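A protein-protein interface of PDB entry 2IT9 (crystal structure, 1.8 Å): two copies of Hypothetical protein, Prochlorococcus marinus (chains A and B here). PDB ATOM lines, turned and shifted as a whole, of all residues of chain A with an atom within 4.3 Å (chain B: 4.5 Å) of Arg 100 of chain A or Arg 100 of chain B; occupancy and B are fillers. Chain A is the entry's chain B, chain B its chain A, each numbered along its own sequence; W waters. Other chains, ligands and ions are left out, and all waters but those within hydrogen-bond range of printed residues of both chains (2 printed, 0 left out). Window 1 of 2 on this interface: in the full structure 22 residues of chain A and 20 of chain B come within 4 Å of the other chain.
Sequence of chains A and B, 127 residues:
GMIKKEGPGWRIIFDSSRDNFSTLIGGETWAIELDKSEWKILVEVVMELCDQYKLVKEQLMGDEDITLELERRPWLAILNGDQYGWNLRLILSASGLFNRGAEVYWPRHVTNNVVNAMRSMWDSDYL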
ATOM      1  N   PHE A  21      -3.064 -14.081  -6.102  1.00  0.00           N
ATOM      2  CA  PHE A  21      -2.112 -14.375  -7.164  1.00  0.00           C
ATOM      3  C   PHE A  21      -1.880 -15.899  -7.258  1.00  0.00           C
ATOM      4  O   PHE A  21      -0.854 -16.421  -6.826  1.00  0.00           O
ATOM      5  CB  PHE A  21      -0.801 -13.605  -6.934  1.00  0.00           C
ATOM      6  CG  PHE A  21      -0.970 -12.104  -6.936  1.00  0.00           C
ATOM      7  CD1 PHE A  21      -1.208 -11.441  -8.121  1.00  0.00           C
ATOM      8  CD2 PHE A  21      -0.852 -11.368  -5.764  1.00  0.00           C
ATOM      9  CE1 PHE A  21      -1.378 -10.080  -8.157  1.00  0.00           C
ATOM     10  CE2 PHE A  21      -1.019  -9.996  -5.783  1.00  0.00           C
ATOM     11  CZ  PHE A  21      -1.286  -9.350  -6.995  1.00  0.00           C
ATOM     12  N   GLU A  33       3.563 -13.487 -11.040  1.00  0.00           N
ATOM     13  CA  GLU A  33       2.293 -14.051 -10.598  1.00  0.00           C
ATOM     14  C   GLU A  33       1.174 -13.225 -11.218  1.00  0.00           C
ATOM     15  O   GLU A  33       1.331 -12.029 -11.444  1.00  0.00           O
ATOM     16  CB  GLU A  33       2.175 -13.950  -9.076  1.00  0.00           C
ATOM     17  CG  GLU A  33       3.202 -14.726  -8.330  1.00  0.00           C
ATOM     18  CD  GLU A  33       3.012 -14.657  -6.832  1.00  0.00           C
ATOM     19  OE1 GLU A  33       2.417 -13.661  -6.335  1.00  0.00           O
ATOM     20  OE2 GLU A  33       3.495 -15.601  -6.154  1.00  0.00           O
ATOM     21  N   LEU A  34       0.029 -13.841 -11.452  1.00  0.00           N
ATOM     22  CA  LEU A  34      -1.143 -13.150 -12.026  1.00  0.00           C
ATOM     23  C   LEU A  34      -2.390 -13.524 -11.259  1.00  0.00           C
ATOM     24  O   LEU A  34      -2.522 -14.664 -10.803  1.00  0.00           O
ATOM     25  CB  LEU A  34      -1.374 -13.611 -13.458  1.00  0.00           C
ATOM     26  CG  LEU A  34      -0.212 -13.475 -14.425  1.00  0.00           C
ATOM     27  CD1 LEU A  34      -0.570 -14.115 -15.758  1.00  0.00           C
ATOM     28  CD2 LEU A  34       0.262 -12.036 -14.622  1.00  0.00           C
ATOM     29  N   GLU A  38      -6.473 -11.355 -14.598  1.00  0.00           N
ATOM     30  CA  GLU A  38      -5.340 -11.131 -15.488  1.00  0.00           C
ATOM     31  C   GLU A  38      -5.011 -12.355 -16.321  1.00  0.00           C
ATOM     32  O   GLU A  38      -4.674 -12.247 -17.512  1.00  0.00           O
ATOM     33  CB  GLU A  38      -4.101 -10.748 -14.668  1.00  0.00           C
ATOM     34  CG  GLU A  38      -4.202  -9.350 -14.094  1.00  0.00           C
ATOM     35  CD  GLU A  38      -3.119  -9.030 -13.070  1.00  0.00           C
ATOM     36  OE1 GLU A  38      -2.642  -9.956 -12.367  1.00  0.00           O
ATOM     37  OE2 GLU A  38      -2.773  -7.829 -12.961  1.00  0.00           O
ATOM     38  N   LEU A  92       1.996  -5.643 -19.105  1.00  0.00           N
ATOM     39  CA  LEU A  92       0.931  -5.671 -18.091  1.00  0.00           C
ATOM     40  C   LEU A  92       0.936  -4.338 -17.378  1.00  0.00           C
ATOM     41  O   LEU A  92       1.900  -4.023 -16.654  1.00  0.00           O
ATOM     42  CB  LEU A  92       1.209  -6.812 -17.095  1.00  0.00           C
ATOM     43  CG  LEU A  92       0.254  -7.047 -15.926  1.00  0.00           C
ATOM     44  CD1 LEU A  92      -1.184  -7.244 -16.382  1.00  0.00           C
ATOM     45  CD2 LEU A  92       0.717  -8.256 -15.055  1.00  0.00           C
ATOM     46  N   ALA A  94      -0.021  -1.580 -14.686  1.00  0.00           N
ATOM     47  CA  ALA A  94      -0.266  -1.649 -13.264  1.00  0.00           C
ATOM     48  C   ALA A  94      -1.699  -1.334 -12.928  1.00  0.00           C
ATOM     49  O   ALA A  94      -2.348  -0.548 -13.628  1.00  0.00           O
ATOM     50  CB  ALA A  94       0.619  -0.667 -12.529  1.00  0.00           C
ATOM     51  N   PHE A  98      -1.587  -3.698  -5.307  1.00  0.00           N
ATOM     52  CA  PHE A  98      -0.714  -4.858  -5.418  1.00  0.00           C
ATOM     53  C   PHE A  98      -0.290  -5.267  -6.815  1.00  0.00           C
ATOM     54  O   PHE A  98       0.729  -5.951  -6.972  1.00  0.00           O
ATOM     55  CB  PHE A  98      -1.474  -6.045  -4.824  1.00  0.00           C
ATOM     56  CG  PHE A  98      -2.067  -5.765  -3.515  1.00  0.00           C
ATOM     57  CD1 PHE A  98      -1.302  -5.196  -2.497  1.00  0.00           C
ATOM     58  CD2 PHE A  98      -3.386  -6.075  -3.265  1.00  0.00           C
ATOM     59  CE1 PHE A  98      -1.866  -4.926  -1.257  1.00  0.00           C
ATOM     60  CE2 PHE A  98      -3.960  -5.804  -2.031  1.00  0.00           C
ATOM     61  CZ  PHE A  98      -3.198  -5.229  -1.029  1.00  0.00           C
ATOM     62  N   ASN A  99      -1.070  -4.858  -7.825  1.00  0.00           N
ATOM     63  CA  ASN A  99      -0.846  -5.299  -9.184  1.00  0.00           C
ATOM     64  C   ASN A  99       0.177  -4.404  -9.859  1.00  0.00           C
ATOM     65  O   ASN A  99      -0.166  -3.487 -10.604  1.00  0.00           O
ATOM     66  CB  ASN A  99      -2.162  -5.381  -9.965  1.00  0.00           C
ATOM     67  CG  ASN A  99      -3.101  -6.433  -9.397  1.00  0.00           C
ATOM     68  OD1 ASN A  99      -3.391  -6.394  -8.225  1.00  0.00           O
ATOM     69  ND2 ASN A  99      -3.562  -7.368 -10.217  1.00  0.00           N
ATOM     70  N   ARG A 100       1.432  -4.675  -9.535  1.00  0.00           N
ATOM     71  CA  ARG A 100       2.552  -3.971 -10.110  1.00  0.00           C
ATOM     72  C   ARG A 100       2.533  -4.199 -11.602  1.00  0.00           C
ATOM     73  O   ARG A 100       2.124  -5.246 -12.102  1.00  0.00           O
ATOM     74  CB  ARG A 100       3.898  -4.471  -9.521  1.00  0.00           C
ATOM     75  CG  ARG A 100       4.441  -5.765 -10.064  1.00  0.00           C
ATOM     76  CD  ARG A 100       5.718  -6.298  -9.430  1.00  0.00           C
ATOM     77  NE  ARG A 100       5.551  -6.738  -8.041  1.00  0.00           N
ATOM     78  CZ  ARG A 100       5.887  -6.054  -6.954  1.00  0.00           C
ATOM     79  NH1 ARG A 100       6.370  -4.802  -7.000  1.00  0.00           N
ATOM     80  NH2 ARG A 100       5.694  -6.609  -5.769  1.00  0.00           N
ATOM     81  N   GLY A 101       3.007  -3.228 -12.348  1.00  0.00           N
ATOM     82  CA  GLY A 101       3.153  -3.475 -13.770  1.00  0.00           C
ATOM     83  C   GLY A 101       4.347  -4.378 -14.029  1.00  0.00           C
ATOM     84  O   GLY A 101       5.238  -4.555 -13.189  1.00  0.00           O
ATOM     85  N   ALA A 102       4.403  -4.931 -15.227  1.00  0.00           N
ATOM     86  CA  ALA A 102       5.501  -5.792 -15.655  1.00  0.00           C
ATOM     87  C   ALA A 102       5.514  -5.895 -17.170  1.00  0.00           C
ATOM     88  O   ALA A 102       4.524  -5.570 -17.817  1.00  0.00           O
ATOM     89  CB  ALA A 102       5.344  -7.172 -15.049  1.00  0.00           C
ATOM     90  N   PHE B  21       4.019   2.510  -7.725  1.00  0.00           N
ATOM     91  CA  PHE B  21       5.042   1.771  -8.415  1.00  0.00           C
ATOM     92  C   PHE B  21       5.862   2.743  -9.271  1.00  0.00           C
ATOM     93  O   PHE B  21       5.749   2.769 -10.491  1.00  0.00           O
ATOM     94  CB  PHE B  21       4.362   0.678  -9.234  1.00  0.00           C
ATOM     95  CG  PHE B  21       3.684  -0.361  -8.386  1.00  0.00           C
ATOM     96  CD1 PHE B  21       4.451  -1.221  -7.596  1.00  0.00           C
ATOM     97  CD2 PHE B  21       2.292  -0.489  -8.382  1.00  0.00           C
ATOM     98  CE1 PHE B  21       3.853  -2.179  -6.797  1.00  0.00           C
ATOM     99  CE2 PHE B  21       1.673  -1.467  -7.587  1.00  0.00           C
ATOM    100  CZ  PHE B  21       2.449  -2.297  -6.794  1.00  0.00           C
ATOM    101  N   ILE B  32       9.971  -5.292 -14.214  1.00  0.00           N
ATOM    102  CA  ILE B  32       8.951  -5.227 -13.205  1.00  0.00           C
ATOM    103  C   ILE B  32       9.012  -3.864 -12.499  1.00  0.00           C
ATOM    104  O   ILE B  32      10.078  -3.260 -12.366  1.00  0.00           O
ATOM    105  CB  ILE B  32       9.038  -6.348 -12.123  1.00  0.00           C
ATOM    106  CG1 ILE B  32      10.380  -6.309 -11.395  1.00  0.00           C
ATOM    107  CG2 ILE B  32       8.833  -7.722 -12.735  1.00  0.00           C
ATOM    108  CD1 ILE B  32      10.436  -7.305 -10.205  1.00  0.00           C
ATOM    109  N   GLU B  33       7.853  -3.370 -12.119  1.00  0.00           N
ATOM    110  CA  GLU B  33       7.744  -2.093 -11.406  1.00  0.00           C
ATOM    111  C   GLU B  33       7.850  -2.370  -9.911  1.00  0.00           C
ATOM    112  O   GLU B  33       7.405  -3.414  -9.436  1.00  0.00           O
ATOM    113  CB  GLU B  33       6.424  -1.406 -11.702  1.00  0.00           C
ATOM    114  CG  GLU B  33       6.216  -0.999 -13.166  1.00  0.00           C
ATOM    115  CD  GLU B  33       4.862  -0.322 -13.356  1.00  0.00           C
ATOM    116  OE1 GLU B  33       3.982  -0.518 -12.485  1.00  0.00           O
ATOM    117  OE2 GLU B  33       4.688   0.384 -14.352  1.00  0.00           O
ATOM    118  N   LEU B  34       8.425  -1.431  -9.171  1.00  0.00           N
ATOM    119  CA  LEU B  34       8.613  -1.556  -7.728  1.00  0.00           C
ATOM    120  C   LEU B  34       8.131  -0.344  -6.984  1.00  0.00           C
ATOM    121  O   LEU B  34       8.218   0.785  -7.511  1.00  0.00           O
ATOM    122  CB  LEU B  34      10.113  -1.690  -7.406  1.00  0.00           C
ATOM    123  CG  LEU B  34      10.939  -2.790  -8.050  1.00  0.00           C
ATOM    124  CD1 LEU B  34      12.427  -2.662  -7.676  1.00  0.00           C
ATOM    125  CD2 LEU B  34      10.405  -4.183  -7.682  1.00  0.00           C
ATOM    126  N   GLU B  38      10.160  -1.414  -1.619  1.00  0.00           N
ATOM    127  CA  GLU B  38      10.813  -2.525  -2.317  1.00  0.00           C
ATOM    128  C   GLU B  38      12.153  -2.106  -2.978  1.00  0.00           C
ATOM    129  O   GLU B  38      13.128  -2.854  -2.977  1.00  0.00           O
ATOM    130  CB  GLU B  38       9.900  -3.058  -3.414  1.00  0.00           C
ATOM    131  CG  GLU B  38       8.701  -3.777  -2.844  1.00  0.00           C
ATOM    132  CD  GLU B  38       7.644  -4.107  -3.875  1.00  0.00           C
ATOM    133  OE1 GLU B  38       7.562  -3.454  -4.944  1.00  0.00           O
ATOM    134  OE2 GLU B  38       6.868  -5.023  -3.576  1.00  0.00           O
ATOM    135  N   LEU B  92      10.981 -11.869  -5.486  1.00  0.00           N
ATOM    136  CA  LEU B  92      10.188 -10.859  -4.813  1.00  0.00           C
ATOM    137  C   LEU B  92       8.890 -11.487  -4.347  1.00  0.00           C
ATOM    138  O   LEU B  92       8.069 -11.924  -5.152  1.00  0.00           O
ATOM    139  CB  LEU B  92       9.917  -9.726  -5.793  1.00  0.00           C
ATOM    140  CG  LEU B  92       9.126  -8.548  -5.234  1.00  0.00           C
ATOM    141  CD1 LEU B  92       9.775  -7.942  -3.976  1.00  0.00           C
ATOM    142  CD2 LEU B  92       8.977  -7.503  -6.331  1.00  0.00           C
ATOM    143  N   ALA B  94       5.176 -12.062  -2.648  1.00  0.00           N
ATOM    144  CA  ALA B  94       3.886 -11.420  -2.719  1.00  0.00           C
ATOM    145  C   ALA B  94       3.412 -11.051  -1.328  1.00  0.00           C
ATOM    146  O   ALA B  94       3.550  -9.901  -0.922  1.00  0.00           O
ATOM    147  CB  ALA B  94       2.883 -12.339  -3.426  1.00  0.00           C
ATOM    148  N   PHE B  98       0.603  -7.392   0.240  1.00  0.00           N
ATOM    149  CA  PHE B  98       0.757  -8.527  -0.641  1.00  0.00           C
ATOM    150  C   PHE B  98       0.732  -8.119  -2.140  1.00  0.00           C
ATOM    151  O   PHE B  98      -0.227  -8.368  -2.883  1.00  0.00           O
ATOM    152  CB  PHE B  98      -0.283  -9.614  -0.291  1.00  0.00           C
ATOM    153  CG  PHE B  98       0.077 -10.995  -0.786  1.00  0.00           C
ATOM    154  N   ASN B  99       1.816  -7.469  -2.551  1.00  0.00           N
ATOM    155  CA  ASN B  99       2.058  -7.027  -3.937  1.00  0.00           C
ATOM    156  C   ASN B  99       2.359  -8.246  -4.809  1.00  0.00           C
ATOM    157  O   ASN B  99       2.844  -9.224  -4.288  1.00  0.00           O
ATOM    158  CB  ASN B  99       3.306  -6.171  -3.974  1.00  0.00           C
ATOM    159  CG  ASN B  99       3.105  -4.712  -3.529  1.00  0.00           C
ATOM    160  OD1 ASN B  99       2.002  -4.233  -3.305  1.00  0.00           O
ATOM    161  ND2 ASN B  99       4.220  -3.984  -3.474  1.00  0.00           N
ATOM    162  N   ARG B 100       2.088  -8.197  -6.112  1.00  0.00           N
ATOM    163  CA  ARG B 100       2.387  -9.327  -7.040  1.00  0.00           C
ATOM    164  C   ARG B 100       3.801  -9.889  -6.883  1.00  0.00           C
ATOM    165  O   ARG B 100       4.795  -9.158  -6.875  1.00  0.00           O
ATOM    166  CB  ARG B 100       2.190  -8.827  -8.482  1.00  0.00           C
ATOM    167  CG  ARG B 100       2.518  -9.774  -9.590  1.00  0.00           C
ATOM    168  CD  ARG B 100       2.771  -9.061 -10.928  1.00  0.00           C
ATOM    169  NE  ARG B 100       1.840  -7.984 -11.242  1.00  0.00           N
ATOM    170  CZ  ARG B 100       0.575  -8.179 -11.583  1.00  0.00           C
ATOM    171  NH1 ARG B 100       0.060  -9.389 -11.572  1.00  0.00           N
ATOM    172  NH2 ARG B 100      -0.207  -7.149 -11.886  1.00  0.00           N
ATOM    173  N   GLY B 101       3.924 -11.203  -6.820  1.00  0.00           N
ATOM    174  CA  GLY B 101       5.225 -11.831  -6.725  1.00  0.00           C
ATOM    175  C   GLY B 101       5.897 -11.913  -8.068  1.00  0.00           C
ATOM    176  O   GLY B 101       5.252 -11.815  -9.122  1.00  0.00           O
ATOM    177  N   ALA B 102       7.209 -11.990  -8.034  1.00  0.00           N
ATOM    178  CA  ALA B 102       7.994 -12.107  -9.253  1.00  0.00           C
ATOM    179  C   ALA B 102       9.366 -12.724  -8.978  1.00  0.00           C
ATOM    180  O   ALA B 102       9.813 -12.806  -7.829  1.00  0.00           O
ATOM    181  CB  ALA B 102       8.169 -10.743  -9.894  1.00  0.00           C
HETATM  182  O   HOH W   1       4.836 -14.823  -4.016  1.00  0.00           O
HETATM  183  O   HOH W   2       2.397  -0.001 -15.519  1.00  0.00           O
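The backbone carbonyl oxygen (O) of Glu 33 of chain B is in hydrogen-bond range of the guanidinium group (NH1) of Arg 100 of chain A (3.0 Å). The side-chain carboxylate (OE1) of Glu 33 of chain B sits at hydrogen-bond distance from the backbone NH (N) of Gly 101 of chain A. The side-chain carboxylate of Glu 38 of chain B lies within salt-bridge range of the guanidinium group of Arg 100 of chain A (2.7 Å). The guanidinium group (NH1) of Arg 100 of chain B lies within hydrogen-bond range of the backbone carbonyl oxygen (O) of Glu 33 of chain A (2.9 Å). The side-chain carboxylate (OE2) of Glu 38 of chain A is in salt-bridge range of the guanidinium group (NH2) of Arg 100 of chain B. The backbone carbonyl oxygen of Phe 98 of chain A lies within hydrogen-bond range of the backbone NH of Arg 100 of chain B, at 2.8 Å. The guanidinium group (NE) of Arg 100 of chain A lies within hydrogen-bond range of the backbone carbonyl oxygen (O) of Arg 100 of chain B (2.8 Å). The backbone NH (N) of Gly 101 of chain B sits at hydrogen-bond distance from the side-chain carboxylate (OE1) of Glu 33 of chain A (2.9 Å).
The side-chain carboxylate (OE2) of Glu 38 of chain B lies within hydrogen-bond range of the side-chain amide nitrogen (ND2) of Asn 99 of chain B, 2.8 Å away. O of Ala 102 of chain B lies within hydrogen-bond range of N of Leu 92 of chain B, at 2.8 Å. The backbone NH of Asn 99 of chain B is in hydrogen-bond range of the backbone carbonyl oxygen of Ala 94 of chain B (3.4 Å). The side-chain carboxylate of Glu 38 of chain A is in hydrogen-bond range of the side-chain amide nitrogen of Asn 99 of chain A (2.9 Å). O of Ala 102 of chain A lies within hydrogen-bond range of N of Leu 92 of chain A (2.8 Å).
CE2 of Phe 21 of chain A touches C of Asn 99 of chain B (3.9 Å). Phe 21 of chain A touches Arg 100 of chain B. Glu 33 of chain A touches Ala 94 of chain B. Arg 100 of chain B touches Leu 34 of chain A. CD2 of Leu 92 of chain A touches CZ of Arg 100 of chain B, at 3.5 Å. Glu 33 of chain B touches Ala 94 of chain A. Phe 98 of chain A touches Asn 99 of chain B (O to CA, 3.5 Å). CB of Asn 99 of chain A touches NH2 of Arg 100 of chain B (3.3 Å). Leu 92 of chain B touches Arg 100 of chain A. NH2 of Arg 100 of chain A touches CB of Asn 99 of chain B (3.0 Å).
Of the printed residues of chain B, Arg 100 of chain A touches Phe 21 (3.6 Å), Glu 33 (3.0 Å), Glu 38 (2.7 Å), Leu 92 (3.4 Å), Asn 99 (3.0 Å) and Arg 100 (2.8 Å). Of chain A, only Phe 21 (3.6 Å), Glu 33 (2.9 Å), Leu 34 (3.97 Å), Glu 38 (2.9 Å), Leu 92 (3.5 Å), Phe 98 (2.8 Å), Asn 99 (3.3 Å) and Arg 100 (2.8 Å) come within 4 Å of Arg 100 of chain B. Printed residues of chain B within 4 Å of Glu 33 of chain A: Ala 94 (3.2 Å), Arg 100 (2.9 Å) and Gly 101 (2.9 Å). Of the printed residues of chain B, Phe 98 of chain A touches Phe 98, Asn 99 and Arg 100. Of the printed residues of chain B, Leu 92 of chain A touches Arg 100. Printed residues of chain A within 4 Å of Ala 94 of chain B: Glu 33. Of the printed residues of chain A, Glu 38 of chain B touches Arg 100. The nearest printed residue of chain A that does not touch Arg 100 of chain B is Gly 101 of chain A (5.0 Å). The nearest printed residue of chain B that does not touch Gly 101 of chain A is Phe 21 of chain B (4.9 Å).
Hydrophobic or aromatic side chains of chain B that line the printed part of chain A: Phe 21, Leu 92 and Ala 94. Hydrophobic or aromatic side chains of chain A that line the printed part of chain B: Phe 21, Leu 92, Ala 94 and Phe 98. Among the printed residues, 22 pairs touch across the chains.
Glu 33 of chain A touches Ala 94 of chain B, and with the chains exchanged Ala 94 of chain A touches Glu 33 of chain B. Glu 33 of chain A touches Gly 101 of chain B, and with the chains exchanged Gly 101 of chain A touches Glu 33 of chain B. Glu 38 of chain A touches Arg 100 of chain B, and with the chains exchanged Arg 100 of chain A touches Glu 38 of chain B. Phe 98 of chain A touches Asn 99 of chain B, but with the chains exchanged Asn 99 of chain A does not touch Phe 98 of chain B (6.1 Å). Positions printed for both chains: 21, 33, 34, 38, 92, 94, 98, 99, 100, 101 and 102. Of the 22 pairs that touch across the chains among the printed residues, 16 have their exchanged pair printed and touching as well.
Water W2 bridges the side-chain carboxylate of Glu 33 of chain B and the backbone NH of Ala 94 of chain A. Water W1 lies within hydrogen-bond range of OE2 of Glu 33 of chain A (2.6 Å) and N of Ala 94 of chain B (3.1 Å).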
